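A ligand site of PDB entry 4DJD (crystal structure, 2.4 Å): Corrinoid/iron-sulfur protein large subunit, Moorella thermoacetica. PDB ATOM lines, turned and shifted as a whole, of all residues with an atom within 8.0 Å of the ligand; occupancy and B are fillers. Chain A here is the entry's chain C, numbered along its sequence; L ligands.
S3 of the ligand lies close to N of Gly 18 (3.3 Å).
The side-chain sulfur (SG) of Cys 25 binds an iron atom (FE4) of the ligand.
S3 of the ligand sits close to N of Cys 17 (3.1 Å).
FE3 of the ligand is bound by SG of Cys 42, 2.3 Å away.
N of Cys 20 sits close to S4 of the ligand (3.5 Å).
The side-chain sulfur (SG) of Cys 20 is bound to an iron atom (FE1) of the ligand.
SG of Cys 17 is bound to FE2 of the ligand, at 2.3 Å.
S3 of the ligand lies close to N of Asn 16 (3.7 Å).
CB of Pro 13 touches S1 of the ligand, at 3.6 Å.
Lys 15 touches the ligand (CB to S1, 3.7 Å).
Glu 19 touches the ligand.
CD2 of Phe 28 touches S2 of the ligand (3.4 Å).
Pro 43 touches the ligand.
Hydrophobic or aromatic side chains within 4 Å of the ligand: Pro 13, Phe 28 and Pro 43.
11 residues have an atom within 4 Å of the ligand: Pro 13, Lys 15, Asn 16, Cys 17, Gly 18, Glu 19, Cys 20, Cys 25, Phe 28, Cys 42 and Pro 43.
The nearest printed residue that does not touch the ligand is Thr 24 (4.1 Å).
The side-chain sulfur (SG) of Cys 25 sits close to the backbone NH (N) of Asn 16 (3.6 Å).
The side-chain sulfur of Cys 25 sits close to the backbone NH of Lys 14 (3.5 Å).
The side-chain sulfur (SG) of Cys 20 sits close to the backbone carbonyl oxygen (O) of Thr 22 (3.7 Å).
The side-chain sulfur (SG) of Cys 25 sits close to the backbone NH (N) of Lys 15, at 3.5 Å.
The side-chain sulfur of Cys 42 lies close to the backbone NH of Tyr 44 (3.6 Å).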
ATOM      1  N   TYR A   9      -1.730  21.449   9.231  1.00  0.00           N
ATOM      2  CA  TYR A   9      -0.841  20.589   8.454  1.00  0.00           C
ATOM      3  C   TYR A   9       0.389  20.101   9.224  1.00  0.00           C
ATOM      4  O   TYR A   9       0.644  18.894   9.277  1.00  0.00           O
ATOM      5  CB  TYR A   9      -0.397  21.295   7.172  1.00  0.00           C
ATOM      6  CG  TYR A   9       0.702  20.554   6.439  1.00  0.00           C
ATOM      7  CD1 TYR A   9       0.467  19.295   5.899  1.00  0.00           C
ATOM      8  CD2 TYR A   9       1.960  21.108   6.287  1.00  0.00           C
ATOM      9  CE1 TYR A   9       1.468  18.621   5.227  1.00  0.00           C
ATOM     10  CE2 TYR A   9       2.968  20.445   5.620  1.00  0.00           C
ATOM     11  CZ  TYR A   9       2.711  19.196   5.088  1.00  0.00           C
ATOM     12  OH  TYR A   9       3.712  18.526   4.425  1.00  0.00           O
ATOM     13  N   LEU A  12       0.293  16.674  11.056  1.00  0.00           N
ATOM     14  CA  LEU A  12      -0.255  15.500  10.392  1.00  0.00           C
ATOM     15  C   LEU A  12       0.857  14.544   9.948  1.00  0.00           C
ATOM     16  O   LEU A  12       1.978  14.977   9.684  1.00  0.00           O
ATOM     17  CB  LEU A  12      -1.123  15.929   9.210  1.00  0.00           C
ATOM     18  CG  LEU A  12      -2.367  16.738   9.586  1.00  0.00           C
ATOM     19  CD1 LEU A  12      -3.231  17.043   8.374  1.00  0.00           C
ATOM     20  CD2 LEU A  12      -3.175  15.997  10.647  1.00  0.00           C
ATOM     21  N   PRO A  13       0.553  13.238   9.868  1.00  0.00           N
ATOM     22  CA  PRO A  13       1.536  12.175   9.604  1.00  0.00           C
ATOM     23  C   PRO A  13       2.329  12.330   8.302  1.00  0.00           C
ATOM     24  O   PRO A  13       3.391  11.713   8.188  1.00  0.00           O
ATOM     25  CB  PRO A  13       0.662  10.909   9.522  1.00  0.00           C
ATOM     26  CG  PRO A  13      -0.529  11.229  10.329  1.00  0.00           C
ATOM     27  CD  PRO A  13      -0.789  12.682  10.113  1.00  0.00           C
ATOM     28  N   LYS A  14       1.822  13.114   7.354  1.00  0.00           N
ATOM     29  CA  LYS A  14       2.479  13.302   6.066  1.00  0.00           C
ATOM     30  C   LYS A  14       2.648  11.982   5.301  1.00  0.00           C
ATOM     31  O   LYS A  14       3.714  11.706   4.746  1.00  0.00           O
ATOM     32  CB  LYS A  14       3.823  14.010   6.224  1.00  0.00           C
ATOM     33  N   LYS A  15       1.590  11.174   5.275  1.00  0.00           N
ATOM     34  CA  LYS A  15       1.621   9.889   4.579  1.00  0.00           C
ATOM     35  C   LYS A  15       1.051  10.001   3.168  1.00  0.00           C
ATOM     36  O   LYS A  15       1.507   9.318   2.250  1.00  0.00           O
ATOM     37  CB  LYS A  15       0.822   8.841   5.354  1.00  0.00           C
ATOM     38  CG  LYS A  15       1.323   8.573   6.766  1.00  0.00           C
ATOM     39  CD  LYS A  15       2.763   8.108   6.781  1.00  0.00           C
ATOM     40  CE  LYS A  15       3.108   7.418   8.092  1.00  0.00           C
ATOM     41  NZ  LYS A  15       2.638   8.208   9.270  1.00  0.00           N
ATOM     42  N   ASN A  16       0.040  10.859   3.020  1.00  0.00           N
ATOM     43  CA  ASN A  16      -0.723  10.975   1.772  1.00  0.00           C
ATOM     44  C   ASN A  16      -1.384   9.654   1.383  1.00  0.00           C
ATOM     45  O   ASN A  16      -1.405   9.278   0.210  1.00  0.00           O
ATOM     46  CB  ASN A  16       0.146  11.510   0.628  1.00  0.00           C
ATOM     47  N   CYS A  17      -1.929   8.953   2.378  1.00  0.00           N
ATOM     48  CA  CYS A  17      -2.573   7.666   2.139  1.00  0.00           C
ATOM     49  C   CYS A  17      -3.993   7.786   1.589  1.00  0.00           C
ATOM     50  O   CYS A  17      -4.508   6.857   0.972  1.00  0.00           O
ATOM     51  CB  CYS A  17      -2.562   6.774   3.387  1.00  0.00           C
ATOM     52  SG  CYS A  17      -2.588   7.597   5.014  1.00  0.00           S
ATOM     53  N   GLY A  18      -4.621   8.934   1.815  1.00  0.00           N
ATOM     54  CA  GLY A  18      -5.948   9.200   1.290  1.00  0.00           C
ATOM     55  C   GLY A  18      -7.051   8.510   2.053  1.00  0.00           C
ATOM     56  O   GLY A  18      -8.199   8.466   1.601  1.00  0.00           O
ATOM     57  N   GLU A  19      -6.725   7.994   3.238  1.00  0.00           N
ATOM     58  CA  GLU A  19      -7.702   7.314   4.079  1.00  0.00           C
ATOM     59  C   GLU A  19      -8.767   8.289   4.588  1.00  0.00           C
ATOM     60  O   GLU A  19      -9.886   7.899   4.910  1.00  0.00           O
ATOM     61  CB  GLU A  19      -7.012   6.621   5.252  1.00  0.00           C
ATOM     62  N   CYS A  20      -8.392   9.566   4.658  1.00  0.00           N
ATOM     63  CA  CYS A  20      -9.294  10.614   5.124  1.00  0.00           C
ATOM     64  C   CYS A  20     -10.236  11.084   4.026  1.00  0.00           C
ATOM     65  O   CYS A  20     -11.031  12.012   4.233  1.00  0.00           O
ATOM     66  CB  CYS A  20      -8.481  11.800   5.647  1.00  0.00           C
ATOM     67  SG  CYS A  20      -7.248  12.398   4.465  1.00  0.00           S
ATOM     68  N   GLY A  21     -10.163  10.445   2.863  1.00  0.00           N
ATOM     69  CA  GLY A  21     -10.969  10.839   1.728  1.00  0.00           C
ATOM     70  C   GLY A  21     -10.392  12.066   1.057  1.00  0.00           C
ATOM     71  O   GLY A  21     -11.103  12.856   0.427  1.00  0.00           O
ATOM     72  N   THR A  22      -9.077  12.226   1.190  1.00  0.00           N
ATOM     73  CA  THR A  22      -8.374  13.370   0.618  1.00  0.00           C
ATOM     74  C   THR A  22      -6.995  12.924   0.139  1.00  0.00           C
ATOM     75  O   THR A  22      -6.256  12.306   0.896  1.00  0.00           O
ATOM     76  CB  THR A  22      -8.213  14.491   1.661  1.00  0.00           C
ATOM     77  OG1 THR A  22      -9.466  14.709   2.331  1.00  0.00           O
ATOM     78  CG2 THR A  22      -7.752  15.779   1.010  1.00  0.00           C
ATOM     79  N   PRO A  23      -6.656  13.253  -1.122  1.00  0.00           N
ATOM     80  CA  PRO A  23      -5.407  12.846  -1.791  1.00  0.00           C
ATOM     81  C   PRO A  23      -4.152  12.968  -0.915  1.00  0.00           C
ATOM     82  O   PRO A  23      -3.370  12.021  -0.846  1.00  0.00           O
ATOM     83  CB  PRO A  23      -5.325  13.788  -3.000  1.00  0.00           C
ATOM     84  CG  PRO A  23      -6.461  14.785  -2.831  1.00  0.00           C
ATOM     85  CD  PRO A  23      -7.480  14.073  -2.016  1.00  0.00           C
ATOM     86  N   THR A  24      -3.973  14.117  -0.264  1.00  0.00           N
ATOM     87  CA  THR A  24      -2.822  14.310   0.617  1.00  0.00           C
ATOM     88  C   THR A  24      -3.231  14.883   1.973  1.00  0.00           C
ATOM     89  O   THR A  24      -4.409  15.182   2.201  1.00  0.00           O
ATOM     90  CB  THR A  24      -1.756  15.243  -0.006  1.00  0.00           C
ATOM     91  OG1 THR A  24      -2.302  16.565  -0.144  1.00  0.00           O
ATOM     92  CG2 THR A  24      -1.315  14.725  -1.368  1.00  0.00           C
ATOM     93  N   CYS A  25      -2.268  15.025   2.865  1.00  0.00           N
ATOM     94  CA  CYS A  25      -2.506  15.644   4.168  1.00  0.00           C
ATOM     95  C   CYS A  25      -2.652  17.145   4.002  1.00  0.00           C
ATOM     96  O   CYS A  25      -3.496  17.772   4.644  1.00  0.00           O
ATOM     97  CB  CYS A  25      -1.350  15.342   5.130  1.00  0.00           C
ATOM     98  SG  CYS A  25      -0.839  13.623   5.183  1.00  0.00           S
ATOM     99  N   LEU A  26      -1.803  17.710   3.156  1.00  0.00           N
ATOM    100  CA  LEU A  26      -1.810  19.154   2.909  1.00  0.00           C
ATOM    101  C   LEU A  26      -3.167  19.574   2.367  1.00  0.00           C
ATOM    102  O   LEU A  26      -3.694  20.630   2.743  1.00  0.00           O
ATOM    103  CB  LEU A  26      -0.699  19.526   1.920  1.00  0.00           C
ATOM    104  CG  LEU A  26      -0.365  21.017   1.789  1.00  0.00           C
ATOM    105  CD1 LEU A  26       0.134  21.568   3.120  1.00  0.00           C
ATOM    106  CD2 LEU A  26       0.675  21.244   0.706  1.00  0.00           C
ATOM    107  N   ALA A  27      -3.737  18.753   1.490  1.00  0.00           N
ATOM    108  CA  ALA A  27      -5.059  19.013   0.935  1.00  0.00           C
ATOM    109  C   ALA A  27      -6.151  18.768   1.973  1.00  0.00           C
ATOM    110  O   ALA A  27      -7.227  19.354   1.892  1.00  0.00           O
ATOM    111  CB  ALA A  27      -5.285  18.164  -0.301  1.00  0.00           C
ATOM    112  N   PHE A  28      -5.865  17.895   2.942  1.00  0.00           N
ATOM    113  CA  PHE A  28      -6.817  17.584   3.994  1.00  0.00           C
ATOM    114  C   PHE A  28      -6.759  18.622   5.114  1.00  0.00           C
ATOM    115  O   PHE A  28      -7.753  18.900   5.776  1.00  0.00           O
ATOM    116  CB  PHE A  28      -6.576  16.182   4.552  1.00  0.00           C
ATOM    117  CG  PHE A  28      -7.505  15.796   5.672  1.00  0.00           C
ATOM    118  CD1 PHE A  28      -8.878  15.846   5.497  1.00  0.00           C
ATOM    119  CD2 PHE A  28      -7.003  15.368   6.894  1.00  0.00           C
ATOM    120  CE1 PHE A  28      -9.731  15.480   6.514  1.00  0.00           C
ATOM    121  CE2 PHE A  28      -7.856  15.007   7.920  1.00  0.00           C
ATOM    122  CZ  PHE A  28      -9.223  15.059   7.732  1.00  0.00           C
ATOM    123  N   ALA A  29      -5.575  19.194   5.313  1.00  0.00           N
ATOM    124  CA  ALA A  29      -5.401  20.256   6.294  1.00  0.00           C
ATOM    125  C   ALA A  29      -6.138  21.498   5.827  1.00  0.00           C
ATOM    126  O   ALA A  29      -6.818  22.172   6.604  1.00  0.00           O
ATOM    127  CB  ALA A  29      -3.932  20.557   6.497  1.00  0.00           C
ATOM    128  N   LEU A  32      -9.679  20.846   6.231  1.00  0.00           N
ATOM    129  CA  LEU A  32     -10.084  21.003   7.619  1.00  0.00           C
ATOM    130  C   LEU A  32     -10.336  22.467   7.975  1.00  0.00           C
ATOM    131  O   LEU A  32     -11.276  22.780   8.717  1.00  0.00           O
ATOM    132  CB  LEU A  32      -9.020  20.408   8.560  1.00  0.00           C
ATOM    133  CG  LEU A  32      -9.279  18.974   9.048  1.00  0.00           C
ATOM    134  CD1 LEU A  32      -7.978  18.291   9.408  1.00  0.00           C
ATOM    135  CD2 LEU A  32     -10.225  18.997  10.239  1.00  0.00           C
ATOM    136  N   LEU A  39     -11.521  15.964  12.078  1.00  0.00           N
ATOM    137  CA  LEU A  39     -10.133  15.618  12.338  1.00  0.00           C
ATOM    138  C   LEU A  39     -10.004  14.134  12.676  1.00  0.00           C
ATOM    139  O   LEU A  39      -8.910  13.570  12.634  1.00  0.00           O
ATOM    140  CB  LEU A  39      -9.552  16.476  13.474  1.00  0.00           C
ATOM    141  CG  LEU A  39     -10.176  16.359  14.872  1.00  0.00           C
ATOM    142  CD1 LEU A  39      -9.157  16.756  15.928  1.00  0.00           C
ATOM    143  CD2 LEU A  39     -11.422  17.230  14.996  1.00  0.00           C
ATOM    144  N   ASP A  40     -11.129  13.506  13.011  1.00  0.00           N
ATOM    145  CA  ASP A  40     -11.154  12.083  13.327  1.00  0.00           C
ATOM    146  C   ASP A  40     -11.106  11.238  12.064  1.00  0.00           C
ATOM    147  O   ASP A  40     -11.012  10.016  12.133  1.00  0.00           O
ATOM    148  CB  ASP A  40     -12.408  11.742  14.142  1.00  0.00           C
ATOM    149  N   SER A  41     -11.175  11.895  10.910  1.00  0.00           N
ATOM    150  CA  SER A  41     -11.115  11.189   9.624  1.00  0.00           C
ATOM    151  C   SER A  41      -9.711  10.679   9.320  1.00  0.00           C
ATOM    152  O   SER A  41      -9.523   9.864   8.424  1.00  0.00           O
ATOM    153  CB  SER A  41     -11.614  12.093   8.496  1.00  0.00           C
ATOM    154  N   CYS A  42      -8.722  11.177  10.063  1.00  0.00           N
ATOM    155  CA  CYS A  42      -7.360  10.664   9.961  1.00  0.00           C
ATOM    156  C   CYS A  42      -7.083   9.680  11.094  1.00  0.00           C
ATOM    157  O   CYS A  42      -7.084  10.062  12.266  1.00  0.00           O
ATOM    158  CB  CYS A  42      -6.339  11.797   9.999  1.00  0.00           C
ATOM    159  SG  CYS A  42      -4.624  11.221   9.910  1.00  0.00           S
ATOM    160  N   PRO A  43      -6.848   8.413  10.745  1.00  0.00           N
ATOM    161  CA  PRO A  43      -6.627   7.355  11.750  1.00  0.00           C
ATOM    162  C   PRO A  43      -5.293   7.500  12.478  1.00  0.00           C
ATOM    163  O   PRO A  43      -5.166   7.022  13.599  1.00  0.00           O
ATOM    164  CB  PRO A  43      -6.636   6.076  10.908  1.00  0.00           C
ATOM    165  CG  PRO A  43      -6.190   6.520   9.553  1.00  0.00           C
ATOM    166  CD  PRO A  43      -6.770   7.894   9.369  1.00  0.00           C
ATOM    167  N   TYR A  44      -4.327   8.150  11.840  1.00  0.00           N
ATOM    168  CA  TYR A  44      -2.987   8.240  12.417  1.00  0.00           C
ATOM    169  C   TYR A  44      -2.803   9.513  13.230  1.00  0.00           C
ATOM    170  O   TYR A  44      -3.745   9.984  13.874  1.00  0.00           O
ATOM    171  CB  TYR A  44      -1.918   8.161  11.312  1.00  0.00           C
ATOM    172  CG  TYR A  44      -1.988   6.926  10.442  1.00  0.00           C
ATOM    173  CD1 TYR A  44      -2.744   5.815  10.812  1.00  0.00           C
ATOM    174  CD2 TYR A  44      -1.282   6.860   9.239  1.00  0.00           C
ATOM    175  CE1 TYR A  44      -2.809   4.697  10.007  1.00  0.00           C
ATOM    176  CE2 TYR A  44      -1.333   5.744   8.433  1.00  0.00           C
ATOM    177  CZ  TYR A  44      -2.103   4.658   8.825  1.00  0.00           C
ATOM    178  OH  TYR A  44      -2.161   3.547   8.016  1.00  0.00           O
ATOM    179  N   VAL A  45      -1.585  10.067  13.202  1.00  0.00           N
ATOM    180  CA  VAL A  45      -1.218  11.278  13.947  1.00  0.00           C
ATOM    181  C   VAL A  45      -1.203  11.085  15.459  1.00  0.00           C
ATOM    182  O   VAL A  45      -2.052  10.383  16.015  1.00  0.00           O
ATOM    183  CB  VAL A  45      -2.089  12.500  13.562  1.00  0.00           C
HETATM  184 FE1  LIG L   1      -5.243  11.694   5.276  1.00  0.00          FE
HETATM  185 FE2  LIG L   1      -3.409   9.665   5.510  1.00  0.00          FE
HETATM  186 FE3  LIG L   1      -4.090  11.172   7.697  1.00  0.00          FE
HETATM  187 FE4  LIG L   1      -2.601  12.272   5.686  1.00  0.00          FE
HETATM  188  S1  LIG L   1      -1.989  10.561   7.061  1.00  0.00           S
HETATM  189  S2  LIG L   1      -4.390  13.217   6.735  1.00  0.00           S
HETATM  190  S3  LIG L   1      -3.502  11.239   3.863  1.00  0.00           S
HETATM  191  S4  LIG L   1      -5.462   9.786   6.511  1.00  0.00           S
